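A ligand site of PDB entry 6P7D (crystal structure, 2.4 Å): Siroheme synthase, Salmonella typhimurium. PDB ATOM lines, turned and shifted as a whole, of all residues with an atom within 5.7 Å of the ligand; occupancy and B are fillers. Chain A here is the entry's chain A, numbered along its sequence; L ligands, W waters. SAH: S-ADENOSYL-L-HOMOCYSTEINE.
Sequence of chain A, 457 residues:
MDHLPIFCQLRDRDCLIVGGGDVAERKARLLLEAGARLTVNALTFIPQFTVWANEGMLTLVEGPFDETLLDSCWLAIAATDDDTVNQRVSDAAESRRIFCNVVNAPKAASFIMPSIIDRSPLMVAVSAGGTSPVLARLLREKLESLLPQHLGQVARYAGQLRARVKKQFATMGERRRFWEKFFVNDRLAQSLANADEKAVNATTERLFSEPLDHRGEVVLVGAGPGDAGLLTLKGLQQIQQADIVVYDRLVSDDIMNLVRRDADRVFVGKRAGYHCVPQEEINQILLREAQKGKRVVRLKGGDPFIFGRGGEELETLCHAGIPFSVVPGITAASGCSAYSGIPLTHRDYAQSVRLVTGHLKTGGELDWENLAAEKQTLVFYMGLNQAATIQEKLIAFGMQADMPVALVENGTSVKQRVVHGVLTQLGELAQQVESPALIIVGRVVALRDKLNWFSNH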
ATOM      1  N   PRO A 225      22.955  11.832   0.985  1.00  0.00           N
ATOM      2  CA  PRO A 225      22.913  10.474   1.565  1.00  0.00           C
ATOM      3  C   PRO A 225      22.787  10.419   3.070  1.00  0.00           C
ATOM      4  O   PRO A 225      22.666   9.314   3.609  1.00  0.00           O
ATOM      5  CB  PRO A 225      24.255   9.881   1.128  1.00  0.00           C
ATOM      6  CG  PRO A 225      25.171  11.090   0.980  1.00  0.00           C
ATOM      7  CD  PRO A 225      24.286  12.213   0.490  1.00  0.00           C
ATOM      8  N   GLY A 226      22.779  11.545   3.783  1.00  0.00           N
ATOM      9  CA  GLY A 226      22.643  11.455   5.224  1.00  0.00           C
ATOM     10  C   GLY A 226      23.299  12.607   5.959  1.00  0.00           C
ATOM     11  O   GLY A 226      22.615  13.363   6.644  1.00  0.00           O
ATOM     12  N   LEU A 250      14.487   7.671   4.545  1.00  0.00           N
ATOM     13  CA  LEU A 250      15.880   7.839   4.158  1.00  0.00           C
ATOM     14  C   LEU A 250      16.311   9.305   4.135  1.00  0.00           C
ATOM     15  O   LEU A 250      17.273   9.646   3.441  1.00  0.00           O
ATOM     16  CB  LEU A 250      16.137   7.207   2.789  1.00  0.00           C
ATOM     17  CG  LEU A 250      16.203   5.680   2.736  1.00  0.00           C
ATOM     18  CD1 LEU A 250      16.731   5.199   1.389  1.00  0.00           C
ATOM     19  CD2 LEU A 250      17.045   5.137   3.892  1.00  0.00           C
ATOM     20  N   GLY A 301      15.854  11.299  -0.061  1.00  0.00           N
ATOM     21  CA  GLY A 301      17.242  10.945   0.190  1.00  0.00           C
ATOM     22  C   GLY A 301      18.032  10.809  -1.094  1.00  0.00           C
ATOM     23  O   GLY A 301      17.504  10.439  -2.141  1.00  0.00           O
ATOM     24  N   GLY A 302      19.325  11.109  -1.013  1.00  0.00           N
ATOM     25  CA  GLY A 302      20.145  11.104  -2.214  1.00  0.00           C
ATOM     26  C   GLY A 302      19.714  12.175  -3.210  1.00  0.00           C
ATOM     27  O   GLY A 302      19.432  13.328  -2.821  1.00  0.00           O
ATOM     28  N   ASP A 303      19.667  11.802  -4.496  1.00  0.00           N
ATOM     29  CA  ASP A 303      19.226  12.642  -5.616  1.00  0.00           C
ATOM     30  C   ASP A 303      17.844  12.198  -6.103  1.00  0.00           C
ATOM     31  O   ASP A 303      17.651  10.994  -6.359  1.00  0.00           O
ATOM     32  CB  ASP A 303      20.246  12.543  -6.750  1.00  0.00           C
ATOM     33  CG  ASP A 303      19.930  13.471  -7.923  1.00  0.00           C
ATOM     34  OD1 ASP A 303      19.154  13.067  -8.829  1.00  0.00           O
ATOM     35  OD2 ASP A 303      20.479  14.594  -7.954  1.00  0.00           O
ATOM     36  N   PRO A 304      16.893  13.124  -6.311  1.00  0.00           N
ATOM     37  CA  PRO A 304      15.503  12.715  -6.623  1.00  0.00           C
ATOM     38  C   PRO A 304      15.323  11.943  -7.929  1.00  0.00           C
ATOM     39  O   PRO A 304      14.303  11.265  -8.075  1.00  0.00           O
ATOM     40  CB  PRO A 304      14.744  14.048  -6.660  1.00  0.00           C
ATOM     41  CG  PRO A 304      15.634  15.047  -5.975  1.00  0.00           C
ATOM     42  CD  PRO A 304      17.032  14.595  -6.278  1.00  0.00           C
ATOM     43  N   ILE A 306      17.574   9.653  -9.406  1.00  0.00           N
ATOM     44  CA  ILE A 306      18.341   8.412  -9.501  1.00  0.00           C
ATOM     45  C   ILE A 306      17.647   7.404  -8.590  1.00  0.00           C
ATOM     46  O   ILE A 306      17.711   7.519  -7.362  1.00  0.00           O
ATOM     47  CB  ILE A 306      19.810   8.601  -9.123  1.00  0.00           C
ATOM     48  CG1 ILE A 306      20.516   9.386 -10.218  1.00  0.00           C
ATOM     49  CG2 ILE A 306      20.497   7.239  -8.937  1.00  0.00           C
ATOM     50  CD1 ILE A 306      21.869   9.882  -9.825  1.00  0.00           C
ATOM     51  N   PHE A 307      16.967   6.427  -9.206  1.00  0.00           N
ATOM     52  CA  PHE A 307      16.184   5.441  -8.473  1.00  0.00           C
ATOM     53  C   PHE A 307      15.275   6.130  -7.449  1.00  0.00           C
ATOM     54  O   PHE A 307      15.117   5.677  -6.318  1.00  0.00           O
ATOM     55  CB  PHE A 307      17.118   4.415  -7.813  1.00  0.00           C
ATOM     56  CG  PHE A 307      17.894   3.596  -8.788  1.00  0.00           C
ATOM     57  CD1 PHE A 307      17.252   2.961  -9.840  1.00  0.00           C
ATOM     58  CD2 PHE A 307      19.274   3.467  -8.664  1.00  0.00           C
ATOM     59  CE1 PHE A 307      17.969   2.191 -10.749  1.00  0.00           C
ATOM     60  CE2 PHE A 307      19.995   2.691  -9.583  1.00  0.00           C
ATOM     61  CZ  PHE A 307      19.340   2.057 -10.625  1.00  0.00           C
ATOM     62  N   GLY A 308      14.705   7.259  -7.863  1.00  0.00           N
ATOM     63  CA  GLY A 308      14.006   8.109  -6.927  1.00  0.00           C
ATOM     64  C   GLY A 308      12.517   7.862  -6.918  1.00  0.00           C
ATOM     65  O   GLY A 308      11.821   8.268  -5.978  1.00  0.00           O
ATOM     66  N   ARG A 309      12.028   7.192  -7.947  1.00  0.00           N
ATOM     67  CA  ARG A 309      10.599   7.005  -8.225  1.00  0.00           C
ATOM     68  C   ARG A 309       9.889   8.335  -8.474  1.00  0.00           C
ATOM     69  O   ARG A 309       8.651   8.368  -8.520  1.00  0.00           O
ATOM     70  CB  ARG A 309       9.906   6.237  -7.098  1.00  0.00           C
ATOM     71  CG  ARG A 309      10.753   5.142  -6.444  1.00  0.00           C
ATOM     72  CD  ARG A 309      11.371   4.203  -7.479  1.00  0.00           C
ATOM     73  NE  ARG A 309      11.551   2.842  -6.973  1.00  0.00           N
ATOM     74  CZ  ARG A 309      12.731   2.308  -6.667  1.00  0.00           C
ATOM     75  NH1 ARG A 309      13.835   3.025  -6.790  1.00  0.00           N
ATOM     76  NH2 ARG A 309      12.802   1.063  -6.217  1.00  0.00           N
ATOM     77  N   ILE A 330      23.344  14.999  -3.634  1.00  0.00           N
ATOM     78  CA  ILE A 330      24.418  14.015  -3.676  1.00  0.00           C
ATOM     79  C   ILE A 330      23.793  12.626  -3.652  1.00  0.00           C
ATOM     80  O   ILE A 330      23.077  12.272  -2.702  1.00  0.00           O
ATOM     81  CB  ILE A 330      25.361  14.195  -2.485  1.00  0.00           C
ATOM     82  CG1 ILE A 330      25.827  15.645  -2.289  1.00  0.00           C
ATOM     83  CG2 ILE A 330      26.572  13.269  -2.664  1.00  0.00           C
ATOM     84  CD1 ILE A 330      26.722  16.193  -3.372  1.00  0.00           C
ATOM     85  N   THR A 331      24.075  11.837  -4.676  1.00  0.00           N
ATOM     86  CA  THR A 331      23.582  10.467  -4.682  1.00  0.00           C
ATOM     87  C   THR A 331      24.388   9.574  -3.724  1.00  0.00           C
ATOM     88  O   THR A 331      25.520   9.878  -3.349  1.00  0.00           O
ATOM     89  CB  THR A 331      23.633   9.899  -6.121  1.00  0.00           C
ATOM     90  OG1 THR A 331      22.933   8.649  -6.162  1.00  0.00           O
ATOM     91  CG2 THR A 331      25.075   9.721  -6.556  1.00  0.00           C
ATOM     92  N   ALA A 332      23.766   8.476  -3.288  1.00  0.00           N
ATOM     93  CA  ALA A 332      24.431   7.598  -2.326  1.00  0.00           C
ATOM     94  C   ALA A 332      25.764   7.082  -2.855  1.00  0.00           C
ATOM     95  O   ALA A 332      26.733   6.946  -2.101  1.00  0.00           O
ATOM     96  CB  ALA A 332      23.511   6.431  -1.942  1.00  0.00           C
ATOM     97  N   ALA A 333      25.836   6.840  -4.180  1.00  0.00           N
ATOM     98  CA  ALA A 333      27.085   6.386  -4.792  1.00  0.00           C
ATOM     99  C   ALA A 333      28.230   7.378  -4.564  1.00  0.00           C
ATOM    100  O   ALA A 333      29.298   7.001  -4.079  1.00  0.00           O
ATOM    101  CB  ALA A 333      26.891   6.144  -6.283  1.00  0.00           C
ATOM    102  N   CYS A 336      28.886   7.721  -0.626  1.00  0.00           N
ATOM    103  CA  CYS A 336      29.582   6.570  -0.036  1.00  0.00           C
ATOM    104  C   CYS A 336      30.977   6.403  -0.630  1.00  0.00           C
ATOM    105  O   CYS A 336      31.910   5.996   0.076  1.00  0.00           O
ATOM    106  CB  CYS A 336      28.770   5.303  -0.248  1.00  0.00           C
ATOM    107  SG  CYS A 336      27.172   5.250   0.568  1.00  0.00           S
ATOM    108  N   PHE A 380      25.392  -1.190  -6.614  1.00  0.00           N
ATOM    109  CA  PHE A 380      24.059  -1.763  -6.442  1.00  0.00           C
ATOM    110  C   PHE A 380      23.310  -1.012  -5.354  1.00  0.00           C
ATOM    111  O   PHE A 380      23.740  -0.997  -4.193  1.00  0.00           O
ATOM    112  CB  PHE A 380      24.141  -3.253  -6.099  1.00  0.00           C
ATOM    113  CG  PHE A 380      24.628  -4.075  -7.230  1.00  0.00           C
ATOM    114  CD1 PHE A 380      25.978  -4.299  -7.387  1.00  0.00           C
ATOM    115  CD2 PHE A 380      23.743  -4.584  -8.165  1.00  0.00           C
ATOM    116  CE1 PHE A 380      26.442  -5.036  -8.448  1.00  0.00           C
ATOM    117  CE2 PHE A 380      24.199  -5.325  -9.237  1.00  0.00           C
ATOM    118  CZ  PHE A 380      25.557  -5.546  -9.373  1.00  0.00           C
ATOM    119  N   TYR A 381      22.173  -0.429  -5.736  1.00  0.00           N
ATOM    120  CA  TYR A 381      21.233   0.207  -4.838  1.00  0.00           C
ATOM    121  C   TYR A 381      20.204  -0.832  -4.419  1.00  0.00           C
ATOM    122  O   TYR A 381      19.701  -1.567  -5.283  1.00  0.00           O
ATOM    123  CB  TYR A 381      20.544   1.374  -5.528  1.00  0.00           C
ATOM    124  CG  TYR A 381      21.389   2.621  -5.681  1.00  0.00           C
ATOM    125  CD1 TYR A 381      22.463   2.678  -6.598  1.00  0.00           C
ATOM    126  CD2 TYR A 381      21.127   3.728  -4.895  1.00  0.00           C
ATOM    127  CE1 TYR A 381      23.219   3.838  -6.708  1.00  0.00           C
ATOM    128  CE2 TYR A 381      21.863   4.861  -4.988  1.00  0.00           C
ATOM    129  CZ  TYR A 381      22.908   4.944  -5.881  1.00  0.00           C
ATOM    130  OH  TYR A 381      23.601   6.139  -5.927  1.00  0.00           O
ATOM    131  N   MET A 382      19.904  -0.881  -3.121  1.00  0.00           N
ATOM    132  CA  MET A 382      18.915  -1.795  -2.518  1.00  0.00           C
ATOM    133  C   MET A 382      19.012  -3.219  -3.063  1.00  0.00           C
ATOM    134  O   MET A 382      18.030  -3.846  -3.426  1.00  0.00           O
ATOM    135  CB  MET A 382      17.485  -1.239  -2.667  1.00  0.00           C
ATOM    136  CG  MET A 382      16.948  -1.053  -4.086  1.00  0.00           C
ATOM    137  SD  MET A 382      15.693   0.243  -4.230  1.00  0.00           S
ATOM    138  CE  MET A 382      16.009   0.792  -5.907  1.00  0.00           C
ATOM    139  N   GLY A 383      20.231  -3.749  -3.089  1.00  0.00           N
ATOM    140  CA  GLY A 383      20.436  -5.130  -3.491  1.00  0.00           C
ATOM    141  C   GLY A 383      20.857  -6.034  -2.347  1.00  0.00           C
ATOM    142  O   GLY A 383      21.419  -7.117  -2.572  1.00  0.00           O
ATOM    143  N   VAL A 408      28.790  -0.486   2.044  1.00  0.00           N
ATOM    144  CA  VAL A 408      28.710   0.727   2.848  1.00  0.00           C
ATOM    145  C   VAL A 408      27.300   0.828   3.405  1.00  0.00           C
ATOM    146  O   VAL A 408      26.331   0.965   2.651  1.00  0.00           O
ATOM    147  CB  VAL A 408      29.062   1.958   2.017  1.00  0.00           C
ATOM    148  CG1 VAL A 408      29.137   3.200   2.922  1.00  0.00           C
ATOM    149  CG2 VAL A 408      30.376   1.707   1.275  1.00  0.00           C
ATOM    150  N   GLU A 409      27.181   0.774   4.739  1.00  0.00           N
ATOM    151  CA  GLU A 409      25.910   0.964   5.424  1.00  0.00           C
ATOM    152  C   GLU A 409      25.873   2.343   6.074  1.00  0.00           C
ATOM    153  O   GLU A 409      26.850   2.753   6.725  1.00  0.00           O
ATOM    154  CB  GLU A 409      25.694  -0.110   6.500  1.00  0.00           C
ATOM    155  CG  GLU A 409      24.342   0.000   7.208  1.00  0.00           C
ATOM    156  CD  GLU A 409      24.215  -0.910   8.411  1.00  0.00           C
ATOM    157  OE1 GLU A 409      23.170  -0.850   9.118  1.00  0.00           O
ATOM    158  OE2 GLU A 409      25.159  -1.700   8.653  1.00  0.00           O
ATOM    159  N   ASN A 410      24.774   3.073   5.888  1.00  0.00           N
ATOM    160  CA  ASN A 410      24.620   4.376   6.532  1.00  0.00           C
ATOM    161  C   ASN A 410      25.729   5.347   6.113  1.00  0.00           C
ATOM    162  O   ASN A 410      26.232   6.123   6.932  1.00  0.00           O
ATOM    163  CB  ASN A 410      24.570   4.237   8.056  1.00  0.00           C
ATOM    164  CG  ASN A 410      23.227   3.727   8.558  1.00  0.00           C
ATOM    165  OD1 ASN A 410      22.178   4.216   8.144  1.00  0.00           O
ATOM    166  ND2 ASN A 410      23.272   2.759   9.480  1.00  0.00           N
ATOM    167  N   GLY A 411      26.142   5.275   4.842  1.00  0.00           N
ATOM    168  CA  GLY A 411      27.154   6.150   4.284  1.00  0.00           C
ATOM    169  C   GLY A 411      26.979   7.620   4.614  1.00  0.00           C
ATOM    170  O   GLY A 411      25.876   8.187   4.462  1.00  0.00           O
ATOM    171  N   THR A 412      28.065   8.245   5.075  1.00  0.00           N
ATOM    172  CA  THR A 412      28.209   9.643   5.453  1.00  0.00           C
ATOM    173  C   THR A 412      27.631   9.941   6.842  1.00  0.00           C
ATOM    174  O   THR A 412      27.861  11.030   7.366  1.00  0.00           O
ATOM    175  CB  THR A 412      27.611  10.643   4.432  1.00  0.00           C
ATOM    176  OG1 THR A 412      26.171  10.680   4.551  1.00  0.00           O
ATOM    177  CG2 THR A 412      28.013  10.272   2.978  1.00  0.00           C
ATOM    178  N   SER A 435      19.850  -2.604   5.849  1.00  0.00           N
ATOM    179  CA  SER A 435      19.489  -1.436   5.044  1.00  0.00           C
ATOM    180  C   SER A 435      19.530  -0.176   5.911  1.00  0.00           C
ATOM    181  O   SER A 435      19.296  -0.245   7.135  1.00  0.00           O
ATOM    182  CB  SER A 435      18.099  -1.618   4.434  1.00  0.00           C
ATOM    183  OG  SER A 435      18.123  -2.482   3.316  1.00  0.00           O
ATOM    184  N   PRO A 436      19.820   0.986   5.316  1.00  0.00           N
ATOM    185  CA  PRO A 436      20.177   1.230   3.907  1.00  0.00           C
ATOM    186  C   PRO A 436      21.648   0.959   3.603  1.00  0.00           C
ATOM    187  O   PRO A 436      22.522   1.333   4.392  1.00  0.00           O
ATOM    188  CB  PRO A 436      19.840   2.716   3.709  1.00  0.00           C
ATOM    189  CG  PRO A 436      20.063   3.326   5.087  1.00  0.00           C
ATOM    190  CD  PRO A 436      19.726   2.241   6.094  1.00  0.00           C
ATOM    191  N   ALA A 437      21.946   0.338   2.466  1.00  0.00           N
ATOM    192  CA  ALA A 437      23.334  -0.031   2.223  1.00  0.00           C
ATOM    193  C   ALA A 437      23.593  -0.106   0.722  1.00  0.00           C
ATOM    194  O   ALA A 437      22.698  -0.448  -0.054  1.00  0.00           O
ATOM    195  CB  ALA A 437      23.686  -1.360   2.910  1.00  0.00           C
ATOM    196  N   LEU A 438      24.804   0.268   0.329  1.00  0.00           N
ATOM    197  CA  LEU A 438      25.265   0.131  -1.051  1.00  0.00           C
ATOM    198  C   LEU A 438      26.234  -1.036  -1.151  1.00  0.00           C
ATOM    199  O   LEU A 438      27.036  -1.276  -0.244  1.00  0.00           O
ATOM    200  CB  LEU A 438      25.998   1.392  -1.533  1.00  0.00           C
ATOM    201  CG  LEU A 438      25.245   2.575  -2.108  1.00  0.00           C
ATOM    202  CD1 LEU A 438      26.211   3.414  -2.920  1.00  0.00           C
ATOM    203  CD2 LEU A 438      24.045   2.137  -2.950  1.00  0.00           C
HETATM  204  N   SAH L   1      17.596   8.246  -4.668  1.00  0.00           N
HETATM  205  CA  SAH L   1      18.583   7.933  -3.642  1.00  0.00           C
HETATM  206  CB  SAH L   1      18.468   6.464  -3.243  1.00  0.00           C
HETATM  207  CG  SAH L   1      17.063   5.892  -3.280  1.00  0.00           C
HETATM  208  SD  SAH L   1      16.985   4.086  -3.491  1.00  0.00           S
HETATM  209  C   SAH L   1      20.012   8.253  -4.094  1.00  0.00           C
HETATM  210  O   SAH L   1      20.247   8.979  -5.067  1.00  0.00           O
HETATM  211  OXT SAH L   1      20.990   7.804  -3.494  1.00  0.00           O
HETATM  212  C5' SAH L   1      17.417   3.688  -1.780  1.00  0.00           C
HETATM  213  C4' SAH L   1      18.693   2.861  -1.718  1.00  0.00           C
HETATM  214  O4' SAH L   1      19.863   3.678  -1.812  1.00  0.00           O
HETATM  215  C3' SAH L   1      18.834   2.047  -0.439  1.00  0.00           C
HETATM  216  O3' SAH L   1      18.268   0.765  -0.586  1.00  0.00           O
HETATM  217  C2' SAH L   1      20.326   1.927  -0.285  1.00  0.00           C
HETATM  218  O2' SAH L   1      20.770   0.832  -1.063  1.00  0.00           O
HETATM  219  C1' SAH L   1      20.872   3.161  -0.968  1.00  0.00           C
HETATM  220  N9  SAH L   1      21.282   4.193   0.020  1.00  0.00           N
HETATM  221  C8  SAH L   1      20.621   5.349   0.304  1.00  0.00           C
HETATM  222  N7  SAH L   1      21.303   6.023   1.250  1.00  0.00           N
HETATM  223  C5  SAH L   1      22.397   5.306   1.608  1.00  0.00           C
HETATM  224  C6  SAH L   1      23.427   5.540   2.521  1.00  0.00           C
HETATM  225  N6  SAH L   1      23.473   6.637   3.271  1.00  0.00           N
HETATM  226  N1  SAH L   1      24.438   4.603   2.646  1.00  0.00           N
HETATM  227  C2  SAH L   1      24.410   3.461   1.872  1.00  0.00           C
HETATM  228  N3  SAH L   1      23.383   3.239   0.970  1.00  0.00           N
HETATM  229  C4  SAH L   1      22.403   4.150   0.831  1.00  0.00           C
HETATM  230  O   HOH W   1      19.748  -1.511   1.280  1.00  0.00           O
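The backbone carbonyl oxygen (O) of Phe 307 sits close to a sulfur (SD) of the ligand (3.7 Å). Residues that only touch the ligand: Leu 250 (3.6 Å), Gly 302 (3.4 Å), Tyr 381 (3.3 Å), Val 408 (3.2 Å), Asn 410 (3.6 Å) and Pro 436 (3.8 Å). 18 residues have an atom within 4 Å of the ligand: Pro 225, Leu 250, Gly 301, Gly 302, Asp 303, Ile 306, Phe 307, Thr 331, Ala 332, Cys 336, Tyr 381, Met 382, Val 408, Asn 410, Gly 411, Pro 436, Ala 437 and Leu 438. The nearest printed residue that does not touch the ligand is Gly 308 (4.2 Å).
Water W1 lies within hydrogen-bond range of OG of Ser 435, N of Ala 437 and O3' of the ligand.
The backbone carbonyl oxygen of Ala 437 lies within hydrogen-bond range of an oxygen (O2') of the ligand (2.5 Å). The backbone carbonyl oxygen of Ile 306 lies within hydrogen-bond range of a nitrogen (N) of the ligand (2.8 Å). N of Met 382 sits at hydrogen-bond distance from O2' of the ligand, at 2.8 Å. The backbone carbonyl oxygen of Pro 225 sits at hydrogen-bond distance from a nitrogen (N6) of the ligand. N of Gly 411 is in hydrogen-bond range of N1 of the ligand (2.9 Å). The backbone carbonyl oxygen of Gly 411 sits at hydrogen-bond distance from a nitrogen (N6) of the ligand (3.1 Å). N of Ala 332 sits at hydrogen-bond distance from OXT of the ligand, 2.9 Å away. OG1 of Thr 331 is in hydrogen-bond range of O of the ligand, 2.9 Å away. The backbone NH of Asp 303 lies within hydrogen-bond range of an oxygen (O) of the ligand (2.9 Å). A nitrogen (N) of the ligand is in hydrogen-bond range of the backbone carbonyl oxygen (O) of Asp 303 (3.2 Å). A nitrogen (N) of the ligand sits close to the backbone carbonyl oxygen (O) of Gly 301, 3.3 Å away. The backbone NH (N) of Leu 438 is in hydrogen-bond range of a nitrogen (N3) of the ligand (3.4 Å). SG of Cys 336 sits at hydrogen-bond distance from N1 of the ligand, 3.5 Å away.
The side-chain sulfur (SD) of Met 382 lies close to the guanidinium group (NH2) of Arg 309, 3.6 Å away. The side-chain sulfur of Cys 336 lies within hydrogen-bond range of the backbone carbonyl oxygen of Ala 332 (3.2 Å). The side-chain hydroxyl of Thr 331 lies within hydrogen-bond range of the side-chain hydroxyl of Tyr 381, at 2.6 Å. The backbone NH (N) of Leu 438 is in hydrogen-bond range of the backbone carbonyl oxygen (O) of Val 408. The backbone NH of Ala 333 sits at hydrogen-bond distance from the side-chain hydroxyl of Tyr 381, at 2.9 Å. N of Asn 410 sits at hydrogen-bond distance from O of Pro 436 (3.2 Å). O of Phe 307 sits at hydrogen-bond distance from NH1 of Arg 309.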
